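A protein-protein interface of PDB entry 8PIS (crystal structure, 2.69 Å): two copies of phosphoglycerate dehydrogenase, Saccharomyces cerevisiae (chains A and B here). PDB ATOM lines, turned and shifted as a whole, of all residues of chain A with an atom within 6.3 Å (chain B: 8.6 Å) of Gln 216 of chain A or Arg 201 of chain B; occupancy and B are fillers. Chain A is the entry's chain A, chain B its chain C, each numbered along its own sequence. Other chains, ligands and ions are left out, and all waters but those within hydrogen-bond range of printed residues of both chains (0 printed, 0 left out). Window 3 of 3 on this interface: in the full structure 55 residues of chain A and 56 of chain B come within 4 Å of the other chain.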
ATOM      1  N   SER A 160     -30.707  -6.989  21.981  1.00  0.00           N
ATOM      2  CA  SER A 160     -30.059  -6.697  20.706  1.00  0.00           C
ATOM      3  C   SER A 160     -29.556  -5.260  20.646  1.00  0.00           C
ATOM      4  O   SER A 160     -28.367  -5.017  20.391  1.00  0.00           O
ATOM      5  CB  SER A 160     -31.036  -6.967  19.567  1.00  0.00           C
ATOM      6  OG  SER A 160     -31.407  -8.332  19.568  1.00  0.00           O
ATOM      7  N   ARG A 161     -30.450  -4.295  20.895  1.00  0.00           N
ATOM      8  CA  ARG A 161     -30.082  -2.885  20.790  1.00  0.00           C
ATOM      9  C   ARG A 161     -28.936  -2.537  21.729  1.00  0.00           C
ATOM     10  O   ARG A 161     -27.995  -1.835  21.338  1.00  0.00           O
ATOM     11  CB  ARG A 161     -31.291  -2.000  21.095  1.00  0.00           C
ATOM     12  CG  ARG A 161     -31.006  -0.508  21.004  1.00  0.00           C
ATOM     13  CD  ARG A 161     -30.806  -0.051  19.575  1.00  0.00           C
ATOM     14  NE  ARG A 161     -30.518   1.371  19.492  1.00  0.00           N
ATOM     15  CZ  ARG A 161     -30.286   2.018  18.356  1.00  0.00           C
ATOM     16  NH1 ARG A 161     -30.357   1.376  17.200  1.00  0.00           N
ATOM     17  NH2 ARG A 161     -30.022   3.309  18.375  1.00  0.00           N
ATOM     18  N   SER A 162     -28.989  -3.039  22.967  1.00  0.00           N
ATOM     19  CA  SER A 162     -28.001  -2.658  23.971  1.00  0.00           C
ATOM     20  C   SER A 162     -26.609  -3.152  23.601  1.00  0.00           C
ATOM     21  O   SER A 162     -25.621  -2.428  23.783  1.00  0.00           O
ATOM     22  CB  SER A 162     -28.421  -3.183  25.346  1.00  0.00           C
ATOM     23  OG  SER A 162     -29.622  -2.566  25.801  1.00  0.00           O
ATOM     24  N   ALA A 164     -25.632  -3.753  20.510  1.00  0.00           N
ATOM     25  CA  ALA A 164     -25.218  -3.038  19.304  1.00  0.00           C
ATOM     26  C   ALA A 164     -24.648  -1.668  19.647  1.00  0.00           C
ATOM     27  O   ALA A 164     -23.560  -1.301  19.188  1.00  0.00           O
ATOM     28  CB  ALA A 164     -26.390  -2.904  18.336  1.00  0.00           C
ATOM     29  N   GLU A 165     -25.355  -0.897  20.472  1.00  0.00           N
ATOM     30  CA  GLU A 165     -24.808   0.392  20.871  1.00  0.00           C
ATOM     31  C   GLU A 165     -23.500   0.207  21.624  1.00  0.00           C
ATOM     32  O   GLU A 165     -22.565   1.001  21.463  1.00  0.00           O
ATOM     33  CB  GLU A 165     -25.813   1.168  21.717  1.00  0.00           C
ATOM     34  CG  GLU A 165     -27.031   1.574  20.926  1.00  0.00           C
ATOM     35  CD  GLU A 165     -28.042   2.340  21.740  1.00  0.00           C
ATOM     36  OE1 GLU A 165     -27.823   2.516  22.966  1.00  0.00           O
ATOM     37  OE2 GLU A 165     -29.071   2.731  21.148  1.00  0.00           O
ATOM     38  N   TYR A 210     -24.363 -12.512  11.592  1.00  0.00           N
ATOM     39  CA  TYR A 210     -25.188 -11.392  11.168  1.00  0.00           C
ATOM     40  C   TYR A 210     -26.639 -11.633  11.569  1.00  0.00           C
ATOM     41  O   TYR A 210     -27.524 -11.634  10.710  1.00  0.00           O
ATOM     42  CB  TYR A 210     -25.049 -11.208   9.657  1.00  0.00           C
ATOM     43  CG  TYR A 210     -25.532  -9.889   9.064  1.00  0.00           C
ATOM     44  CD1 TYR A 210     -24.759  -8.736   9.175  1.00  0.00           C
ATOM     45  CD2 TYR A 210     -26.714  -9.808   8.338  1.00  0.00           C
ATOM     46  CE1 TYR A 210     -25.159  -7.538   8.609  1.00  0.00           C
ATOM     47  CE2 TYR A 210     -27.128  -8.605   7.771  1.00  0.00           C
ATOM     48  CZ  TYR A 210     -26.345  -7.475   7.911  1.00  0.00           C
ATOM     49  OH  TYR A 210     -26.748  -6.277   7.352  1.00  0.00           O
ATOM     50  N   GLY A 211     -26.887 -11.866  12.855  1.00  0.00           N
ATOM     51  CA  GLY A 211     -28.216 -12.172  13.409  1.00  0.00           C
ATOM     52  C   GLY A 211     -28.901 -10.943  13.975  1.00  0.00           C
ATOM     53  O   GLY A 211     -28.765  -9.831  13.445  1.00  0.00           O
ATOM     54  N   HIS A 212     -29.625 -11.137  15.084  1.00  0.00           N
ATOM     55  CA  HIS A 212     -30.359 -10.034  15.710  1.00  0.00           C
ATOM     56  C   HIS A 212     -29.440  -8.885  16.102  1.00  0.00           C
ATOM     57  O   HIS A 212     -29.712  -7.721  15.785  1.00  0.00           O
ATOM     58  CB  HIS A 212     -31.154 -10.543  16.913  1.00  0.00           C
ATOM     59  CG  HIS A 212     -32.363 -11.332  16.525  1.00  0.00           C
ATOM     60  ND1 HIS A 212     -32.311 -12.675  16.218  1.00  0.00           N
ATOM     61  CD2 HIS A 212     -33.656 -10.962  16.379  1.00  0.00           C
ATOM     62  CE1 HIS A 212     -33.522 -13.099  15.902  1.00  0.00           C
ATOM     63  NE2 HIS A 212     -34.357 -12.080  15.996  1.00  0.00           N
ATOM     64  N   ILE A 213     -28.354  -9.180  16.805  1.00  0.00           N
ATOM     65  CA  ILE A 213     -27.433  -8.115  17.182  1.00  0.00           C
ATOM     66  C   ILE A 213     -26.649  -7.632  15.968  1.00  0.00           C
ATOM     67  O   ILE A 213     -26.539  -6.428  15.718  1.00  0.00           O
ATOM     68  CB  ILE A 213     -26.502  -8.589  18.305  1.00  0.00           C
ATOM     69  CG1 ILE A 213     -27.329  -8.868  19.559  1.00  0.00           C
ATOM     70  CG2 ILE A 213     -25.429  -7.551  18.545  1.00  0.00           C
ATOM     71  CD1 ILE A 213     -26.610  -9.583  20.656  1.00  0.00           C
ATOM     72  N   GLY A 214     -26.114  -8.561  15.182  1.00  0.00           N
ATOM     73  CA  GLY A 214     -25.262  -8.165  14.073  1.00  0.00           C
ATOM     74  C   GLY A 214     -25.974  -7.296  13.055  1.00  0.00           C
ATOM     75  O   GLY A 214     -25.466  -6.249  12.640  1.00  0.00           O
ATOM     76  N   SER A 215     -27.168  -7.714  12.640  1.00  0.00           N
ATOM     77  CA  SER A 215     -27.877  -6.956  11.620  1.00  0.00           C
ATOM     78  C   SER A 215     -28.232  -5.568  12.135  1.00  0.00           C
ATOM     79  O   SER A 215     -28.189  -4.585  11.386  1.00  0.00           O
ATOM     80  CB  SER A 215     -29.108  -7.733  11.154  1.00  0.00           C
ATOM     81  OG  SER A 215     -30.036  -7.959  12.198  1.00  0.00           O
ATOM     82  N   GLN A 216     -28.558  -5.465  13.420  1.00  0.00           N
ATOM     83  CA  GLN A 216     -28.828  -4.158  13.999  1.00  0.00           C
ATOM     84  C   GLN A 216     -27.539  -3.363  14.189  1.00  0.00           C
ATOM     85  O   GLN A 216     -27.524  -2.142  14.000  1.00  0.00           O
ATOM     86  CB  GLN A 216     -29.608  -4.345  15.295  1.00  0.00           C
ATOM     87  CG  GLN A 216     -30.128  -3.085  15.926  1.00  0.00           C
ATOM     88  CD  GLN A 216     -31.143  -3.398  17.016  1.00  0.00           C
ATOM     89  OE1 GLN A 216     -31.446  -4.566  17.292  1.00  0.00           O
ATOM     90  NE2 GLN A 216     -31.700  -2.354  17.617  1.00  0.00           N
ATOM     91  N   LEU A 217     -26.442  -4.035  14.552  1.00  0.00           N
ATOM     92  CA  LEU A 217     -25.155  -3.347  14.582  1.00  0.00           C
ATOM     93  C   LEU A 217     -24.769  -2.837  13.199  1.00  0.00           C
ATOM     94  O   LEU A 217     -24.128  -1.781  13.080  1.00  0.00           O
ATOM     95  CB  LEU A 217     -24.072  -4.264  15.148  1.00  0.00           C
ATOM     96  CG  LEU A 217     -22.660  -3.659  15.228  1.00  0.00           C
ATOM     97  CD1 LEU A 217     -22.592  -2.416  16.104  1.00  0.00           C
ATOM     98  CD2 LEU A 217     -21.678  -4.687  15.741  1.00  0.00           C
ATOM     99  N   SER A 218     -25.144  -3.575  12.150  1.00  0.00           N
ATOM    100  CA  SER A 218     -24.816  -3.181  10.783  1.00  0.00           C
ATOM    101  C   SER A 218     -25.358  -1.796  10.461  1.00  0.00           C
ATOM    102  O   SER A 218     -24.639  -0.950   9.918  1.00  0.00           O
ATOM    103  CB  SER A 218     -25.364  -4.209   9.798  1.00  0.00           C
ATOM    104  OG  SER A 218     -25.071  -3.825   8.469  1.00  0.00           O
ATOM    105  N   VAL A 219     -26.638  -1.555  10.775  1.00  0.00           N
ATOM    106  CA  VAL A 219     -27.282  -0.281  10.454  1.00  0.00           C
ATOM    107  C   VAL A 219     -26.644   0.858  11.241  1.00  0.00           C
ATOM    108  O   VAL A 219     -26.410   1.948  10.705  1.00  0.00           O
ATOM    109  CB  VAL A 219     -28.791  -0.368  10.746  1.00  0.00           C
ATOM    110  CG1 VAL A 219     -29.473   0.978  10.485  1.00  0.00           C
ATOM    111  CG2 VAL A 219     -29.420  -1.464   9.947  1.00  0.00           C
ATOM    112  N   LEU A 220     -26.353   0.624  12.523  1.00  0.00           N
ATOM    113  CA  LEU A 220     -25.686   1.640  13.327  1.00  0.00           C
ATOM    114  C   LEU A 220     -24.303   1.949  12.779  1.00  0.00           C
ATOM    115  O   LEU A 220     -23.876   3.112  12.765  1.00  0.00           O
ATOM    116  CB  LEU A 220     -25.576   1.177  14.777  1.00  0.00           C
ATOM    117  CG  LEU A 220     -26.873   1.016  15.559  1.00  0.00           C
ATOM    118  CD1 LEU A 220     -26.594   0.469  16.945  1.00  0.00           C
ATOM    119  CD2 LEU A 220     -27.589   2.342  15.641  1.00  0.00           C
ATOM    120  N   ALA A 221     -23.589   0.910  12.326  1.00  0.00           N
ATOM    121  CA  ALA A 221     -22.215   1.080  11.862  1.00  0.00           C
ATOM    122  C   ALA A 221     -22.146   1.956  10.614  1.00  0.00           C
ATOM    123  O   ALA A 221     -21.336   2.890  10.542  1.00  0.00           O
ATOM    124  CB  ALA A 221     -21.593  -0.288  11.603  1.00  0.00           C
ATOM    125  N   LEU A 239     -28.439  -5.814   5.187  1.00  0.00           N
ATOM    126  CA  LEU A 239     -29.130  -4.573   5.485  1.00  0.00           C
ATOM    127  C   LEU A 239     -28.337  -3.400   4.933  1.00  0.00           C
ATOM    128  O   LEU A 239     -27.102  -3.400   4.963  1.00  0.00           O
ATOM    129  CB  LEU A 239     -29.329  -4.405   6.986  1.00  0.00           C
ATOM    130  CG  LEU A 239     -30.267  -5.407   7.644  1.00  0.00           C
ATOM    131  CD1 LEU A 239     -30.270  -5.128   9.123  1.00  0.00           C
ATOM    132  CD2 LEU A 239     -31.674  -5.310   7.063  1.00  0.00           C
ATOM    133  N   GLU A 358     -33.531  -0.168  29.568  1.00  0.00           N
ATOM    134  CA  GLU A 358     -34.422  -0.541  28.471  1.00  0.00           C
ATOM    135  C   GLU A 358     -34.455  -2.046  28.261  1.00  0.00           C
ATOM    136  O   GLU A 358     -35.534  -2.649  28.183  1.00  0.00           O
ATOM    137  CB  GLU A 358     -34.008   0.170  27.187  1.00  0.00           C
ATOM    138  CG  GLU A 358     -34.328   1.654  27.197  1.00  0.00           C
ATOM    139  CD  GLU A 358     -33.311   2.479  27.959  1.00  0.00           C
ATOM    140  OE1 GLU A 358     -32.276   1.921  28.387  1.00  0.00           O
ATOM    141  OE2 GLU A 358     -33.575   3.678  28.180  1.00  0.00           O
ATOM    142  N   SER A 362     -37.654  -4.391  28.592  1.00  0.00           N
ATOM    143  CA  SER A 362     -38.223  -5.245  27.554  1.00  0.00           C
ATOM    144  C   SER A 362     -38.302  -6.697  28.005  1.00  0.00           C
ATOM    145  O   SER A 362     -39.287  -7.388  27.718  1.00  0.00           O
ATOM    146  CB  SER A 362     -37.420  -5.119  26.262  1.00  0.00           C
ATOM    147  OG  SER A 362     -37.565  -3.818  25.736  1.00  0.00           O
ATOM    148  N   ILE B 171     -21.126   9.831  24.719  1.00  0.00           N
ATOM    149  CA  ILE B 171     -22.525   9.657  25.094  1.00  0.00           C
ATOM    150  C   ILE B 171     -22.779   8.207  25.467  1.00  0.00           C
ATOM    151  O   ILE B 171     -23.354   7.906  26.520  1.00  0.00           O
ATOM    152  CB  ILE B 171     -23.460  10.112  23.962  1.00  0.00           C
ATOM    153  CG1 ILE B 171     -23.458  11.627  23.820  1.00  0.00           C
ATOM    154  CG2 ILE B 171     -24.871   9.585  24.187  1.00  0.00           C
ATOM    155  CD1 ILE B 171     -24.173  12.080  22.583  1.00  0.00           C
ATOM    156  N   ILE B 172     -22.300   7.283  24.632  1.00  0.00           N
ATOM    157  CA  ILE B 172     -22.550   5.871  24.884  1.00  0.00           C
ATOM    158  C   ILE B 172     -21.791   5.400  26.115  1.00  0.00           C
ATOM    159  O   ILE B 172     -22.326   4.638  26.931  1.00  0.00           O
ATOM    160  CB  ILE B 172     -22.213   5.047  23.639  1.00  0.00           C
ATOM    161  CG1 ILE B 172     -23.043   5.556  22.460  1.00  0.00           C
ATOM    162  CG2 ILE B 172     -22.559   3.596  23.892  1.00  0.00           C
ATOM    163  CD1 ILE B 172     -22.624   5.011  21.112  1.00  0.00           C
ATOM    164  N   ALA B 175     -23.569   6.789  29.203  1.00  0.00           N
ATOM    165  CA  ALA B 175     -24.851   6.119  29.378  1.00  0.00           C
ATOM    166  C   ALA B 175     -24.698   4.676  29.847  1.00  0.00           C
ATOM    167  O   ALA B 175     -25.633   4.135  30.442  1.00  0.00           O
ATOM    168  CB  ALA B 175     -25.645   6.154  28.070  1.00  0.00           C
ATOM    169  N   TRP B 198     -28.269   3.218  30.231  1.00  0.00           N
ATOM    170  CA  TRP B 198     -29.302   3.552  29.263  1.00  0.00           C
ATOM    171  C   TRP B 198     -28.910   3.119  27.862  1.00  0.00           C
ATOM    172  O   TRP B 198     -27.751   3.256  27.462  1.00  0.00           O
ATOM    173  CB  TRP B 198     -29.543   5.068  29.251  1.00  0.00           C
ATOM    174  CG  TRP B 198     -29.699   5.623  30.616  1.00  0.00           C
ATOM    175  CD1 TRP B 198     -28.751   6.297  31.339  1.00  0.00           C
ATOM    176  CD2 TRP B 198     -30.843   5.501  31.463  1.00  0.00           C
ATOM    177  NE1 TRP B 198     -29.250   6.628  32.577  1.00  0.00           N
ATOM    178  CE2 TRP B 198     -30.533   6.152  32.679  1.00  0.00           C
ATOM    179  CE3 TRP B 198     -32.106   4.919  31.309  1.00  0.00           C
ATOM    180  CZ2 TRP B 198     -31.442   6.236  33.730  1.00  0.00           C
ATOM    181  CZ3 TRP B 198     -33.005   5.002  32.355  1.00  0.00           C
ATOM    182  CH2 TRP B 198     -32.669   5.655  33.551  1.00  0.00           C
ATOM    183  N   GLU B 199     -29.887   2.616  27.111  1.00  0.00           N
ATOM    184  CA  GLU B 199     -29.801   2.684  25.661  1.00  0.00           C
ATOM    185  C   GLU B 199     -29.863   4.141  25.229  1.00  0.00           C
ATOM    186  O   GLU B 199     -30.664   4.929  25.741  1.00  0.00           O
ATOM    187  CB  GLU B 199     -30.940   1.914  24.993  1.00  0.00           C
ATOM    188  CG  GLU B 199     -30.844   0.405  25.073  1.00  0.00           C
ATOM    189  CD  GLU B 199     -31.998  -0.303  24.360  1.00  0.00           C
ATOM    190  OE1 GLU B 199     -32.962   0.367  23.917  1.00  0.00           O
ATOM    191  OE2 GLU B 199     -31.935  -1.541  24.244  1.00  0.00           O
ATOM    192  N   VAL B 200     -28.998   4.505  24.289  1.00  0.00           N
ATOM    193  CA  VAL B 200     -28.967   5.888  23.824  1.00  0.00           C
ATOM    194  C   VAL B 200     -30.165   6.172  22.925  1.00  0.00           C
ATOM    195  O   VAL B 200     -30.639   7.314  22.847  1.00  0.00           O
ATOM    196  CB  VAL B 200     -27.613   6.148  23.148  1.00  0.00           C
ATOM    197  CG1 VAL B 200     -27.594   7.455  22.430  1.00  0.00           C
ATOM    198  CG2 VAL B 200     -26.544   6.146  24.217  1.00  0.00           C
ATOM    199  N   ARG B 201     -30.707   5.139  22.282  1.00  0.00           N
ATOM    200  CA  ARG B 201     -31.919   5.299  21.494  1.00  0.00           C
ATOM    201  C   ARG B 201     -33.057   5.811  22.371  1.00  0.00           C
ATOM    202  O   ARG B 201     -33.319   5.270  23.450  1.00  0.00           O
ATOM    203  CB  ARG B 201     -32.307   3.966  20.862  1.00  0.00           C
ATOM    204  CG  ARG B 201     -33.598   4.021  20.070  1.00  0.00           C
ATOM    205  CD  ARG B 201     -33.984   2.660  19.551  1.00  0.00           C
ATOM    206  NE  ARG B 201     -34.281   1.726  20.632  1.00  0.00           N
ATOM    207  CZ  ARG B 201     -34.394   0.413  20.455  1.00  0.00           C
ATOM    208  NH1 ARG B 201     -34.223  -0.102  19.238  1.00  0.00           N
ATOM    209  NH2 ARG B 201     -34.666  -0.387  21.484  1.00  0.00           N
ATOM    210  N   GLY B 202     -33.736   6.858  21.902  1.00  0.00           N
ATOM    211  CA  GLY B 202     -34.847   7.443  22.627  1.00  0.00           C
ATOM    212  C   GLY B 202     -34.486   8.587  23.549  1.00  0.00           C
ATOM    213  O   GLY B 202     -35.387   9.281  24.029  1.00  0.00           O
ATOM    214  N   LYS B 203     -33.206   8.797  23.838  1.00  0.00           N
ATOM    215  CA  LYS B 203     -32.828   9.898  24.702  1.00  0.00           C
ATOM    216  C   LYS B 203     -32.689  11.186  23.892  1.00  0.00           C
ATOM    217  O   LYS B 203     -32.680  11.184  22.658  1.00  0.00           O
ATOM    218  CB  LYS B 203     -31.537   9.569  25.440  1.00  0.00           C
ATOM    219  CG  LYS B 203     -31.605   8.276  26.232  1.00  0.00           C
ATOM    220  CD  LYS B 203     -32.653   8.338  27.332  1.00  0.00           C
ATOM    221  CE  LYS B 203     -32.511   7.150  28.279  1.00  0.00           C
ATOM    222  NZ  LYS B 203     -32.743   5.872  27.569  1.00  0.00           N
ATOM    223  N   THR B 204     -32.524  12.295  24.605  1.00  0.00           N
ATOM    224  CA  THR B 204     -32.457  13.618  23.999  1.00  0.00           C
ATOM    225  C   THR B 204     -31.063  14.207  24.175  1.00  0.00           C
ATOM    226  O   THR B 204     -30.542  14.281  25.298  1.00  0.00           O
ATOM    227  CB  THR B 204     -33.503  14.546  24.617  1.00  0.00           C
ATOM    228  OG1 THR B 204     -34.814  14.031  24.358  1.00  0.00           O
ATOM    229  CG2 THR B 204     -33.390  15.937  24.042  1.00  0.00           C
ATOM    230  N   ALA B 221     -26.164  11.924  15.897  1.00  0.00           N
ATOM    231  CA  ALA B 221     -26.990  11.616  17.065  1.00  0.00           C
ATOM    232  C   ALA B 221     -28.336  11.027  16.651  1.00  0.00           C
ATOM    233  O   ALA B 221     -28.810  10.044  17.237  1.00  0.00           O
ATOM    234  CB  ALA B 221     -27.181  12.868  17.917  1.00  0.00           C
ATOM    235  N   GLU B 222     -28.977  11.633  15.649  1.00  0.00           N
ATOM    236  CA  GLU B 222     -30.241  11.098  15.161  1.00  0.00           C
ATOM    237  C   GLU B 222     -30.056   9.692  14.618  1.00  0.00           C
ATOM    238  O   GLU B 222     -30.901   8.817  14.840  1.00  0.00           O
ATOM    239  CB  GLU B 222     -30.812  12.005  14.077  1.00  0.00           C
ATOM    240  CG  GLU B 222     -31.195  13.389  14.552  1.00  0.00           C
ATOM    241  CD  GLU B 222     -31.728  14.253  13.421  1.00  0.00           C
ATOM    242  OE1 GLU B 222     -31.802  13.757  12.272  1.00  0.00           O
ATOM    243  OE2 GLU B 222     -32.032  15.440  13.672  1.00  0.00           O
ATOM    244  N   ALA B 223     -28.955   9.463  13.898  1.00  0.00           N
ATOM    245  CA  ALA B 223     -28.652   8.134  13.374  1.00  0.00           C
ATOM    246  C   ALA B 223     -28.549   7.101  14.488  1.00  0.00           C
ATOM    247  O   ALA B 223     -28.939   5.941  14.307  1.00  0.00           O
ATOM    248  CB  ALA B 223     -27.362   8.180  12.564  1.00  0.00           C
ATOM    249  N   MET B 224     -28.009   7.495  15.638  1.00  0.00           N
ATOM    250  CA  MET B 224     -27.982   6.635  16.816  1.00  0.00           C
ATOM    251  C   MET B 224     -29.321   6.565  17.529  1.00  0.00           C
ATOM    252  O   MET B 224     -29.407   5.919  18.581  1.00  0.00           O
ATOM    253  CB  MET B 224     -26.913   7.123  17.793  1.00  0.00           C
ATOM    254  CG  MET B 224     -25.490   6.939  17.290  1.00  0.00           C
ATOM    255  SD  MET B 224     -25.018   5.205  17.108  1.00  0.00           S
ATOM    256  CE  MET B 224     -25.183   5.018  15.337  1.00  0.00           C
ATOM    257  N   GLY B 225     -30.351   7.223  17.005  1.00  0.00           N
ATOM    258  CA  GLY B 225     -31.670   7.177  17.587  1.00  0.00           C
ATOM    259  C   GLY B 225     -31.955   8.242  18.618  1.00  0.00           C
ATOM    260  O   GLY B 225     -32.951   8.126  19.345  1.00  0.00           O
ATOM    261  N   LEU B 226     -31.132   9.280  18.700  1.00  0.00           N
ATOM    262  CA  LEU B 226     -31.357  10.348  19.661  1.00  0.00           C
ATOM    263  C   LEU B 226     -32.261  11.417  19.056  1.00  0.00           C
ATOM    264  O   LEU B 226     -32.251  11.662  17.845  1.00  0.00           O
ATOM    265  CB  LEU B 226     -30.027  10.970  20.093  1.00  0.00           C
ATOM    266  CG  LEU B 226     -29.086  10.205  21.032  1.00  0.00           C
ATOM    267  CD1 LEU B 226     -27.682  10.703  20.899  1.00  0.00           C
ATOM    268  CD2 LEU B 226     -29.506  10.459  22.446  1.00  0.00           C
ATOM    269  N   HIS B 227     -33.065  12.035  19.917  1.00  0.00           N
ATOM    270  CA  HIS B 227     -33.690  13.315  19.610  1.00  0.00           C
ATOM    271  C   HIS B 227     -32.699  14.439  19.870  1.00  0.00           C
ATOM    272  O   HIS B 227     -31.983  14.427  20.874  1.00  0.00           O
ATOM    273  CB  HIS B 227     -34.933  13.534  20.471  1.00  0.00           C
ATOM    274  CG  HIS B 227     -35.961  12.463  20.324  1.00  0.00           C
ATOM    275  ND1 HIS B 227     -36.706  12.299  19.175  1.00  0.00           N
ATOM    276  CD2 HIS B 227     -36.388  11.511  21.190  1.00  0.00           C
ATOM    277  CE1 HIS B 227     -37.540  11.287  19.339  1.00  0.00           C
ATOM    278  NE2 HIS B 227     -37.369  10.793  20.551  1.00  0.00           N
ATOM    279  N   ASP B 256     -31.349  14.823  27.915  1.00  0.00           N
ATOM    280  CA  ASP B 256     -30.702  13.792  28.709  1.00  0.00           C
ATOM    281  C   ASP B 256     -29.199  13.937  28.647  1.00  0.00           C
ATOM    282  O   ASP B 256     -28.505  13.671  29.641  1.00  0.00           O
ATOM    283  CB  ASP B 256     -31.116  12.418  28.192  1.00  0.00           C
ATOM    284  CG  ASP B 256     -32.577  12.169  28.380  1.00  0.00           C
ATOM    285  OD1 ASP B 256     -33.075  12.481  29.478  1.00  0.00           O
ATOM    286  OD2 ASP B 256     -33.242  11.766  27.404  1.00  0.00           O
ATOM    287  N   PHE B 257     -28.700  14.422  27.514  1.00  0.00           N
ATOM    288  CA  PHE B 257     -27.284  14.656  27.299  1.00  0.00           C
ATOM    289  C   PHE B 257     -27.116  16.098  26.852  1.00  0.00           C
ATOM    290  O   PHE B 257     -27.787  16.536  25.908  1.00  0.00           O
ATOM    291  CB  PHE B 257     -26.707  13.701  26.244  1.00  0.00           C
ATOM    292  CG  PHE B 257     -26.687  12.277  26.669  1.00  0.00           C
ATOM    293  CD1 PHE B 257     -25.632  11.780  27.398  1.00  0.00           C
ATOM    294  CD2 PHE B 257     -27.740  11.437  26.364  1.00  0.00           C
ATOM    295  CE1 PHE B 257     -25.610  10.453  27.790  1.00  0.00           C
ATOM    296  CE2 PHE B 257     -27.731  10.110  26.764  1.00  0.00           C
ATOM    297  CZ  PHE B 257     -26.663   9.620  27.482  1.00  0.00           C
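1 position is printed for both chains.
Of the 13 pairs that touch across the chains among the printed residues, none has its exchanged pair printed and touching as well.
No residue of chain B comes within 4 Å of Gly 214 of chain A.
Ser 215 of chain A touches none of the printed residues of chain B.
Leu 217 of chain A touches none of the printed residues of chain B.
Printed residues of chain B within 4 Å of Glu 358 of chain A: Trp 198 (3.5 Å), Glu 199 (2.8 Å) and Lys 203 (2.4 Å).
Of the printed residues of chain A, Ile 172 of chain B touches Glu 165.
Ala 175 of chain B touches none of the printed residues of chain A.
Of the printed residues of chain A, Val 200 of chain B touches Glu 165.
Of chain A, only Arg 161, Glu 165 and Gln 216 come within 4 Å of Arg 201 of chain B.
Printed residues of chain A within 4 Å of Lys 203 of chain B: Glu 358 (2.4 Å).
Of the printed residues of chain A, Met 224 of chain B touches Arg 161 (2.7 Å) and Leu 220 (3.5 Å).
The nearest printed residue of chain B that does not touch Arg 161 of chain A is Gly 225 of chain B (4.2 Å).
O of Met 224 of chain B lies within hydrogen-bond range of NH2 of Arg 161 of chain A, 2.7 Å away.
The side-chain hydroxyl (OG) of Ser 162 of chain A lies within hydrogen-bond range of the side-chain carboxylate (OE2) of Glu 199 of chain B (3.0 Å).
OE1 of Glu 165 of chain A is in hydrogen-bond range of N of Val 200 of chain B (2.7 Å).
The side-chain carboxylate of Glu 165 of chain A is in hydrogen-bond range of the backbone NH of Arg 201 of chain B (3.1 Å).
The side-chain carboxylate of Glu 358 of chain A lies within hydrogen-bond range of the backbone NH of Glu 199 of chain B (2.8 Å).
OE2 of Glu 358 of chain A is in salt-bridge range of NZ of Lys 203 of chain B (2.4 Å).
OE2 of Glu 199 of chain B touches CB of Arg 161 of chain A (3.2 Å).
CD of Arg 161 of chain A touches NH1 of Arg 201 of chain B, at 3.4 Å.
Ile 172 of chain B touches Glu 165 of chain A (CG2 to O, 3.6 Å).
OE1 of Glu 165 of chain A touches CA of Glu 199 of chain B (3.3 Å).
Gln 216 of chain A touches Arg 201 of chain B (NE2 to NH1, 3.8 Å).
O of Leu 220 of chain A touches CE of Met 224 of chain B (3.5 Å).
OE1 of Glu 358 of chain A touches CA of Trp 198 of chain B, 3.5 Å away.
Hydrophobic or aromatic side chains of chain B within 4 Å of the printed part of chain A: Ile 172, Trp 198, Val 200 and Met 224.
Among the printed residues, 13 pairs touch across the chains.
NE of Arg 161 of chain A lies within salt-bridge range of OE2 of Glu 165 of chain A (2.6 Å).
The side-chain hydroxyl (OG) of Ser 362 of chain A is in hydrogen-bond range of the backbone carbonyl oxygen (O) of Glu 358 of chain A, 3.4 Å away.
The backbone carbonyl oxygen (O) of Ala 175 of chain B is in hydrogen-bond range of the backbone NH (N) of Trp 198 of chain B (2.8 Å).
NH2 of Arg 201 of chain B is in salt-bridge range of OE1 of Glu 199 of chain B, at 3.1 Å.
NZ of Lys 203 of chain B sits at hydrogen-bond distance from O of Glu 199 of chain B (2.9 Å).
The backbone carbonyl oxygen (O) of Lys 203 of chain B sits at hydrogen-bond distance from the backbone NH (N) of His 227 of chain B (2.9 Å).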
